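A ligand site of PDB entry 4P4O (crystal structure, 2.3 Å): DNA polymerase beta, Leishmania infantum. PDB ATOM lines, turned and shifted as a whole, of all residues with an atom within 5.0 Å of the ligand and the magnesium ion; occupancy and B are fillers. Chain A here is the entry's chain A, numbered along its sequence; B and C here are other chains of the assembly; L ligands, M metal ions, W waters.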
ATOM      1  N   GLY A 185     -12.370  -8.054   2.472  1.00  0.00           N
ATOM      2  CA  GLY A 185     -13.390  -8.229   1.459  1.00  0.00           C
ATOM      3  C   GLY A 185     -13.688  -6.930   0.727  1.00  0.00           C
ATOM      4  O   GLY A 185     -12.865  -6.011   0.706  1.00  0.00           O
ATOM      5  N   SER A 186     -14.864  -6.865   0.135  1.00  0.00           N
ATOM      6  CA  SER A 186     -15.254  -5.748  -0.731  1.00  0.00           C
ATOM      7  C   SER A 186     -15.368  -4.468   0.089  1.00  0.00           C
ATOM      8  O   SER A 186     -15.351  -3.361  -0.460  1.00  0.00           O
ATOM      9  CB  SER A 186     -16.565  -6.066  -1.438  1.00  0.00           C
ATOM     10  OG  SER A 186     -17.572  -6.408  -0.485  1.00  0.00           O
ATOM     11  N   ARG A 189     -12.217  -2.790   0.089  1.00  0.00           N
ATOM     12  CA  ARG A 189     -12.099  -2.215  -1.249  1.00  0.00           C
ATOM     13  C   ARG A 189     -13.082  -1.046  -1.466  1.00  0.00           C
ATOM     14  O   ARG A 189     -13.255  -0.575  -2.584  1.00  0.00           O
ATOM     15  CB  ARG A 189     -12.288  -3.271  -2.333  1.00  0.00           C
ATOM     16  CG  ARG A 189     -11.305  -4.425  -2.248  1.00  0.00           C
ATOM     17  CD  ARG A 189     -11.141  -5.138  -3.566  1.00  0.00           C
ATOM     18  NE  ARG A 189     -12.412  -5.539  -4.198  1.00  0.00           N
ATOM     19  CZ  ARG A 189     -13.195  -6.529  -3.778  1.00  0.00           C
ATOM     20  NH1 ARG A 189     -12.877  -7.230  -2.687  1.00  0.00           N
ATOM     21  NH2 ARG A 189     -14.298  -6.819  -4.449  1.00  0.00           N
ATOM     22  N   PHE A 193     -21.672  -1.382  -1.018  1.00  0.00           N
ATOM     23  CA  PHE A 193     -22.321  -2.566  -0.464  1.00  0.00           C
ATOM     24  C   PHE A 193     -21.394  -3.781  -0.523  1.00  0.00           C
ATOM     25  O   PHE A 193     -20.555  -3.908  -1.436  1.00  0.00           O
ATOM     26  CB  PHE A 193     -23.597  -2.887  -1.232  1.00  0.00           C
ATOM     27  CG  PHE A 193     -24.667  -1.832  -1.116  1.00  0.00           C
ATOM     28  CD1 PHE A 193     -24.659  -0.719  -1.959  1.00  0.00           C
ATOM     29  CD2 PHE A 193     -25.690  -1.958  -0.186  1.00  0.00           C
ATOM     30  CE1 PHE A 193     -25.645   0.248  -1.865  1.00  0.00           C
ATOM     31  CE2 PHE A 193     -26.683  -0.985  -0.089  1.00  0.00           C
ATOM     32  CZ  PHE A 193     -26.660   0.120  -0.917  1.00  0.00           C
ATOM     33  N   SER A 194     -21.549  -4.688   0.436  1.00  0.00           N
ATOM     34  CA  SER A 194     -20.805  -5.942   0.461  1.00  0.00           C
ATOM     35  C   SER A 194     -21.742  -7.134   0.609  1.00  0.00           C
ATOM     36  O   SER A 194     -22.805  -7.011   1.207  1.00  0.00           O
ATOM     37  CB  SER A 194     -19.776  -5.925   1.605  1.00  0.00           C
ATOM     38  OG  SER A 194     -18.747  -4.983   1.354  1.00  0.00           O
ATOM     39  N   GLY A 195     -21.345  -8.277   0.062  1.00  0.00           N
ATOM     40  CA  GLY A 195     -22.124  -9.491   0.201  1.00  0.00           C
ATOM     41  C   GLY A 195     -22.022 -10.117   1.587  1.00  0.00           C
ATOM     42  O   GLY A 195     -22.930 -10.823   2.016  1.00  0.00           O
ATOM     43  N   ASP A 196     -20.907  -9.879   2.282  1.00  0.00           N
ATOM     44  CA  ASP A 196     -20.704 -10.491   3.599  1.00  0.00           C
ATOM     45  C   ASP A 196     -19.627  -9.799   4.419  1.00  0.00           C
ATOM     46  O   ASP A 196     -19.133  -8.721   4.053  1.00  0.00           O
ATOM     47  CB  ASP A 196     -20.370 -11.982   3.449  1.00  0.00           C
ATOM     48  CG  ASP A 196     -19.066 -12.223   2.697  1.00  0.00           C
ATOM     49  OD1 ASP A 196     -18.163 -11.383   2.820  1.00  0.00           O
ATOM     50  OD2 ASP A 196     -18.951 -13.252   1.992  1.00  0.00           O
ATOM     51  N   ASP A 198     -15.905 -10.360   5.915  1.00  0.00           N
ATOM     52  CA  ASP A 198     -14.694 -11.165   5.892  1.00  0.00           C
ATOM     53  C   ASP A 198     -13.691 -10.660   6.889  1.00  0.00           C
ATOM     54  O   ASP A 198     -12.974  -9.696   6.622  1.00  0.00           O
ATOM     55  CB  ASP A 198     -14.050 -11.132   4.515  1.00  0.00           C
ATOM     56  CG  ASP A 198     -14.920 -11.728   3.461  1.00  0.00           C
ATOM     57  OD1 ASP A 198     -15.204 -12.940   3.531  1.00  0.00           O
ATOM     58  OD2 ASP A 198     -15.326 -10.981   2.558  1.00  0.00           O
ATOM     59  N   THR A 288      -4.999 -11.578   0.257  1.00  0.00           N
ATOM     60  CA  THR A 288      -5.932 -12.623  -0.164  1.00  0.00           C
ATOM     61  C   THR A 288      -7.388 -12.296   0.189  1.00  0.00           C
ATOM     62  O   THR A 288      -8.265 -12.334  -0.684  1.00  0.00           O
ATOM     63  CB  THR A 288      -5.587 -13.973   0.498  1.00  0.00           C
ATOM     64  OG1 THR A 288      -4.351 -14.443  -0.027  1.00  0.00           O
ATOM     65  CG2 THR A 288      -6.697 -15.002   0.249  1.00  0.00           C
ATOM     66  N   PHE A 289      -7.628 -11.966   1.453  1.00  0.00           N
ATOM     67  CA  PHE A 289      -8.990 -11.765   1.943  1.00  0.00           C
ATOM     68  C   PHE A 289      -9.593 -10.406   1.547  1.00  0.00           C
ATOM     69  O   PHE A 289     -10.791 -10.187   1.683  1.00  0.00           O
ATOM     70  CB  PHE A 289      -9.060 -12.059   3.441  1.00  0.00           C
ATOM     71  CG  PHE A 289      -8.584 -13.451   3.806  1.00  0.00           C
ATOM     72  CD1 PHE A 289      -9.033 -14.554   3.097  1.00  0.00           C
ATOM     73  CD2 PHE A 289      -7.677 -13.642   4.828  1.00  0.00           C
ATOM     74  CE1 PHE A 289      -8.589 -15.836   3.418  1.00  0.00           C
ATOM     75  CE2 PHE A 289      -7.227 -14.916   5.146  1.00  0.00           C
ATOM     76  CZ  PHE A 289      -7.689 -16.022   4.443  1.00  0.00           C
ATOM     77  N   THR A 290      -8.761  -9.508   1.043  1.00  0.00           N
ATOM     78  CA  THR A 290      -9.268  -8.265   0.451  1.00  0.00           C
ATOM     79  C   THR A 290      -9.662  -8.498  -1.005  1.00  0.00           C
ATOM     80  O   THR A 290     -10.664  -7.975  -1.474  1.00  0.00           O
ATOM     81  CB  THR A 290      -8.222  -7.155   0.558  1.00  0.00           C
ATOM     82  OG1 THR A 290      -7.918  -6.930   1.934  1.00  0.00           O
ATOM     83  CG2 THR A 290      -8.715  -5.843  -0.114  1.00  0.00           C
ATOM     84  N   GLY A 291      -8.866  -9.308  -1.708  1.00  0.00           N
ATOM     85  CA  GLY A 291      -9.183  -9.649  -3.086  1.00  0.00           C
ATOM     86  C   GLY A 291      -9.087  -8.407  -3.963  1.00  0.00           C
ATOM     87  O   GLY A 291      -8.232  -7.552  -3.716  1.00  0.00           O
ATOM     88  N   SER A 292      -9.948  -8.283  -4.977  1.00  0.00           N
ATOM     89  CA  SER A 292     -11.009  -9.244  -5.267  1.00  0.00           C
ATOM     90  C   SER A 292     -10.470 -10.590  -5.704  1.00  0.00           C
ATOM     91  O   SER A 292      -9.251 -10.782  -5.871  1.00  0.00           O
ATOM     92  CB  SER A 292     -11.876  -8.713  -6.397  1.00  0.00           C
ATOM     93  OG  SER A 292     -11.174  -8.818  -7.633  1.00  0.00           O
ATOM     94  N   LYS A 293     -11.377 -11.536  -5.910  1.00  0.00           N
ATOM     95  CA  LYS A 293     -11.005 -12.867  -6.345  1.00  0.00           C
ATOM     96  C   LYS A 293     -10.212 -12.867  -7.651  1.00  0.00           C
ATOM     97  O   LYS A 293      -9.189 -13.527  -7.754  1.00  0.00           O
ATOM     98  CB  LYS A 293     -12.253 -13.756  -6.465  1.00  0.00           C
ATOM     99  CG  LYS A 293     -11.980 -15.178  -6.892  1.00  0.00           C
ATOM    100  CD  LYS A 293     -12.185 -15.318  -8.399  1.00  0.00           C
ATOM    101  CE  LYS A 293     -12.352 -16.764  -8.830  1.00  0.00           C
ATOM    102  NZ  LYS A 293     -12.213 -16.909 -10.311  1.00  0.00           N
ATOM    103  N   ASN A 296      -6.815 -11.696  -7.056  1.00  0.00           N
ATOM    104  CA  ASN A 296      -5.964 -12.707  -6.435  1.00  0.00           C
ATOM    105  C   ASN A 296      -5.402 -13.642  -7.467  1.00  0.00           C
ATOM    106  O   ASN A 296      -4.234 -14.020  -7.388  1.00  0.00           O
ATOM    107  CB  ASN A 296      -6.705 -13.511  -5.370  1.00  0.00           C
ATOM    108  CG  ASN A 296      -7.019 -12.696  -4.153  1.00  0.00           C
ATOM    109  OD1 ASN A 296      -6.431 -11.628  -3.977  1.00  0.00           O
ATOM    110  ND2 ASN A 296      -7.931 -13.171  -3.319  1.00  0.00           N
ATOM    111  N   ARG A 300      -1.460 -14.152  -8.297  1.00  0.00           N
ATOM    112  CA  ARG A 300      -0.939 -15.510  -8.162  1.00  0.00           C
ATOM    113  C   ARG A 300      -0.354 -16.069  -9.448  1.00  0.00           C
ATOM    114  O   ARG A 300       0.611 -16.839  -9.408  1.00  0.00           O
ATOM    115  CB  ARG A 300      -2.011 -16.439  -7.591  1.00  0.00           C
ATOM    116  CG  ARG A 300      -2.324 -16.106  -6.127  1.00  0.00           C
ATOM    117  CD  ARG A 300      -3.468 -16.926  -5.515  1.00  0.00           C
ATOM    118  NE  ARG A 300      -3.715 -16.488  -4.142  1.00  0.00           N
ATOM    119  CZ  ARG A 300      -4.395 -17.187  -3.233  1.00  0.00           C
ATOM    120  NH1 ARG A 300      -4.926 -18.363  -3.531  1.00  0.00           N
ATOM    121  NH2 ARG A 300      -4.532 -16.689  -2.007  1.00  0.00           N
ATOM    122  P    DA B   5      -5.525 -20.777 -12.735  1.00  0.00           P
ATOM    123  OP1  DA B   5      -6.744 -21.548 -12.373  1.00  0.00           O
ATOM    124  OP2  DA B   5      -5.660 -19.426 -13.319  1.00  0.00           O
ATOM    125  O5'  DA B   5      -4.618 -20.681 -11.418  1.00  0.00           O
ATOM    126  C5'  DA B   5      -3.818 -19.540 -11.216  1.00  0.00           C
ATOM    127  C4'  DA B   5      -3.398 -19.447  -9.758  1.00  0.00           C
ATOM    128  O4'  DA B   5      -4.470 -18.931  -8.910  1.00  0.00           O
ATOM    129  C3'  DA B   5      -2.954 -20.746  -9.118  1.00  0.00           C
ATOM    130  O3'  DA B   5      -1.872 -20.408  -8.268  1.00  0.00           O
ATOM    131  C2'  DA B   5      -4.205 -21.200  -8.378  1.00  0.00           C
ATOM    132  C1'  DA B   5      -4.840 -19.887  -7.941  1.00  0.00           C
ATOM    133  N9   DA B   5      -6.291 -19.858  -7.963  1.00  0.00           N
ATOM    134  C8   DA B   5      -7.108 -20.372  -8.938  1.00  0.00           C
ATOM    135  N7   DA B   5      -8.392 -20.181  -8.708  1.00  0.00           N
ATOM    136  C5   DA B   5      -8.419 -19.480  -7.511  1.00  0.00           C
ATOM    137  C6   DA B   5      -9.470 -18.956  -6.716  1.00  0.00           C
ATOM    138  N6   DA B   5     -10.767 -19.082  -7.030  1.00  0.00           N
ATOM    139  N1   DA B   5      -9.127 -18.311  -5.575  1.00  0.00           N
ATOM    140  C2   DA B   5      -7.837 -18.179  -5.257  1.00  0.00           C
ATOM    141  N3   DA B   5      -6.778 -18.625  -5.918  1.00  0.00           N
ATOM    142  C4   DA B   5      -7.136 -19.267  -7.040  1.00  0.00           C
ATOM    143  P    DA B   6      -1.021 -21.553  -7.544  1.00  0.00           P
ATOM    144  OP1  DA B   6       0.332 -21.025  -7.298  1.00  0.00           O
ATOM    145  OP2  DA B   6      -1.165 -22.797  -8.328  1.00  0.00           O
ATOM    146  O5'  DA B   6      -1.794 -21.773  -6.174  1.00  0.00           O
ATOM    147  C5'  DA B   6      -1.793 -20.729  -5.246  1.00  0.00           C
ATOM    148  C4'  DA B   6      -2.810 -21.049  -4.187  1.00  0.00           C
ATOM    149  O4'  DA B   6      -4.152 -20.877  -4.706  1.00  0.00           O
ATOM    150  C3'  DA B   6      -2.729 -22.477  -3.616  1.00  0.00           C
ATOM    151  O3'  DA B   6      -2.069 -22.312  -2.344  1.00  0.00           O
ATOM    152  C2'  DA B   6      -4.188 -22.940  -3.553  1.00  0.00           C
ATOM    153  C1'  DA B   6      -4.969 -21.644  -3.846  1.00  0.00           C
ATOM    154  N9   DA B   6      -6.272 -21.876  -4.486  1.00  0.00           N
ATOM    155  C8   DA B   6      -6.502 -22.509  -5.668  1.00  0.00           C
ATOM    156  N7   DA B   6      -7.786 -22.556  -5.973  1.00  0.00           N
ATOM    157  C5   DA B   6      -8.434 -21.927  -4.919  1.00  0.00           C
ATOM    158  C6   DA B   6      -9.800 -21.667  -4.634  1.00  0.00           C
ATOM    159  N6   DA B   6     -10.811 -22.030  -5.442  1.00  0.00           N
ATOM    160  N1   DA B   6     -10.098 -21.015  -3.478  1.00  0.00           N
ATOM    161  C2   DA B   6      -9.079 -20.649  -2.686  1.00  0.00           C
ATOM    162  N3   DA B   6      -7.761 -20.845  -2.844  1.00  0.00           N
ATOM    163  C4   DA B   6      -7.495 -21.495  -3.984  1.00  0.00           C
ATOM    164  P    DT C   6     -19.147 -18.676   0.309  1.00  0.00           P
ATOM    165  OP1  DT C   6     -20.006 -17.713   1.051  1.00  0.00           O
ATOM    166  OP2  DT C   6     -19.336 -18.827  -1.151  1.00  0.00           O
ATOM    167  O5'  DT C   6     -17.611 -18.343   0.568  1.00  0.00           O
ATOM    168  C5'  DT C   6     -17.054 -18.127   1.857  1.00  0.00           C
ATOM    169  C4'  DT C   6     -15.558 -17.853   1.733  1.00  0.00           C
ATOM    170  O4'  DT C   6     -14.887 -19.020   1.189  1.00  0.00           O
ATOM    171  C3'  DT C   6     -15.175 -16.732   0.768  1.00  0.00           C
ATOM    172  C2'  DT C   6     -13.747 -17.096   0.392  1.00  0.00           C
ATOM    173  C1'  DT C   6     -13.728 -18.627   0.500  1.00  0.00           C
ATOM    174  N1   DT C   6     -13.715 -19.345  -0.803  1.00  0.00           N
ATOM    175  C2   DT C   6     -12.480 -19.660  -1.306  1.00  0.00           C
ATOM    176  O2   DT C   6     -11.452 -19.382  -0.733  1.00  0.00           O
ATOM    177  N3   DT C   6     -12.486 -20.345  -2.486  1.00  0.00           N
ATOM    178  C4   DT C   6     -13.599 -20.707  -3.224  1.00  0.00           C
ATOM    179  O4   DT C   6     -13.449 -21.295  -4.283  1.00  0.00           O
ATOM    180  C5   DT C   6     -14.895 -20.349  -2.667  1.00  0.00           C
ATOM    181  C7   DT C   6     -16.159 -20.721  -3.411  1.00  0.00           C
ATOM    182  C6   DT C   6     -14.893 -19.686  -1.486  1.00  0.00           C
HETATM  183  P1  LIG L   1     -15.838 -12.869  -1.150  1.00  0.00           P
HETATM  184  O1  LIG L   1     -16.563 -12.464   0.082  1.00  0.00           O
HETATM  185  O2  LIG L   1     -16.574 -13.999  -1.858  1.00  0.00           O
HETATM  186  O3  LIG L   1     -14.360 -13.389  -0.706  1.00  0.00           O
HETATM  187  C1  LIG L   1     -13.578 -12.784   0.192  1.00  0.00           C
HETATM  188  C2  LIG L   1     -12.192 -12.670  -0.212  1.00  0.00           C
HETATM  189  O4  LIG L   1     -11.694 -14.014  -0.464  1.00  0.00           O
HETATM  190  C3  LIG L   1     -10.999 -14.045  -1.670  1.00  0.00           C
HETATM  191  N1  LIG L   1     -11.379 -15.140  -2.499  1.00  0.00           N
HETATM  192  C4  LIG L   1     -12.686 -15.366  -2.649  1.00  0.00           C
HETATM  193  C5  LIG L   1     -10.492 -15.910  -3.143  1.00  0.00           C
HETATM  194  O5  LIG L   1      -9.260 -15.704  -3.026  1.00  0.00           O
HETATM  195  N2  LIG L   1     -10.886 -16.925  -3.939  1.00  0.00           N
HETATM  196  C6  LIG L   1     -12.190 -17.178  -4.092  1.00  0.00           C
HETATM  197  O6  LIG L   1     -12.616 -18.229  -4.919  1.00  0.00           O
HETATM  198  C7  LIG L   1     -13.142 -16.401  -3.450  1.00  0.00           C
HETATM  199  C8  LIG L   1     -14.646 -16.662  -3.631  1.00  0.00           C
HETATM  200  C9  LIG L   1     -11.279 -12.767  -2.389  1.00  0.00           C
HETATM  201  C10 LIG L   1     -12.112 -11.960  -1.513  1.00  0.00           C
HETATM  202  O7  LIG L   1     -15.719 -11.688  -2.152  1.00  0.00           O
HETATM  203  P2  LIG L   1     -15.762 -10.132  -1.892  1.00  0.00           P
HETATM  204  O8  LIG L   1     -15.527  -9.767  -0.440  1.00  0.00           O
HETATM  205  O9  LIG L   1     -14.694  -9.449  -2.753  1.00  0.00           O
HETATM  206  O10 LIG L   1     -17.217  -9.594  -2.345  1.00  0.00           O
HETATM  207  P3  LIG L   1     -18.556  -9.636  -1.538  1.00  0.00           P
HETATM  208  O11 LIG L   1     -18.454 -10.098  -0.142  1.00  0.00           O
HETATM  209  O12 LIG L   1     -19.496 -10.524  -2.323  1.00  0.00           O
HETATM  210  O13 LIG L   1     -19.107  -8.206  -1.522  1.00  0.00           O
HETATM  211 MG    MG M   1     -16.864 -10.662   1.089  1.00  0.00          MG
HETATM  212  O   HOH W   1     -15.445 -13.258  -4.716  1.00  0.00           O
HETATM  213  O   HOH W   2     -19.689 -12.924  -0.730  1.00  0.00           O
HETATM  214  O   HOH W   3     -14.752 -19.077  -6.588  1.00  0.00           O
HETATM  215  O   HOH W   4     -17.018  -8.460   2.073  1.00  0.00           O
HETATM  216  O   HOH W   5     -14.218 -10.905  -4.873  1.00  0.00           O
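Water W4 lies within hydrogen-bond range of the backbone carbonyl oxygen of Asp 196 (2.9 Å) and the backbone NH of Ser 186 (3.3 Å).
Water W5 bridges O9 of the ligand (2.6 Å) and N of Lys 293 (3.1 Å).
Water W3 lies within hydrogen-bond range of an oxygen (O6) of the ligand and O4 of DT 6 of chain C.
Water W2 bridges OD2 of Asp 196 (2.8 Å) and O12 of the ligand (2.9 Å).
Of the 19 residues printed, 2 come within 4 Å of the magnesium ion.
The magnesium ion is bound by O1 of the ligand (2.1 Å), O11 of the ligand (2.1 Å), OD2 of Asp 198 (2.2 Å), O8 of the ligand (2.2 Å), OD1 of Asp 196 (2.3 Å) and water W4 (2.4 Å).
OG of Ser 194 is in hydrogen-bond range of OG of Ser 186, 2.6 Å away.
The guanidinium group (NH1) of Arg 189 lies within hydrogen-bond range of the backbone carbonyl oxygen (O) of Thr 290, 2.6 Å away.
N3 of DT 6 of chain C lies close to N1 of DA 6 of chain B, 2.7 Å away.
OG1 of Thr 288 is in hydrogen-bond range of NH2 of Arg 300 (3.0 Å).
The side-chain amide nitrogen (ND2) of Asn 296 sits at hydrogen-bond distance from the backbone carbonyl oxygen (O) of Thr 288 (2.8 Å).
The backbone NH (N) of Gly 185 is in hydrogen-bond range of the backbone carbonyl oxygen (O) of Phe 289, 2.8 Å away.
NH1 of Arg 300 is in hydrogen-bond range of N3 of DA 5 of chain B.
N3 of DT 6 of chain C lies close to O6 of the ligand, 3.2 Å away.
Gly 185 touches the ligand (CA to O8, 3.2 Å).
Ser 194 touches the ligand.
Thr 288 touches the ligand (O to C3, 3.4 Å).
O of Phe 289 touches C2 of the ligand, 3.4 Å away.
CA of Gly 291 touches C9 of the ligand (3.8 Å).
CG of Lys 293 touches C6 of the ligand (3.4 Å).
Within 4 Å of the ligand: Gly 185, Ser 186, Arg 189, Ser 194, Gly 195, Asp 196, Asp 198, Thr 288, Phe 289, Gly 291, Lys 293, Asn 296, DA 5 of chain B and DT 6 of chain C.
The nearest printed residue that does not touch the ligand is DA 6 of chain B (4.02 Å).
The guanidinium group of Arg 189 is in salt-bridge range of an oxygen (O9) of the ligand (2.9 Å).
O13 of the ligand lies within hydrogen-bond range of OG of Ser 186 (2.6 Å).
N1 of DA 5 of chain B sits at hydrogen-bond distance from N2 of the ligand, 2.8 Å away.
N of Asp 196 lies close to O11 of the ligand, 3.5 Å away.
An oxygen (O5) of the ligand is in hydrogen-bond range of the side-chain amide nitrogen (ND2) of Asn 296, at 2.9 Å.
O13 of the ligand lies within hydrogen-bond range of N of Gly 195.
N of Ser 186 lies close to O8 of the ligand, 3.0 Å away.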
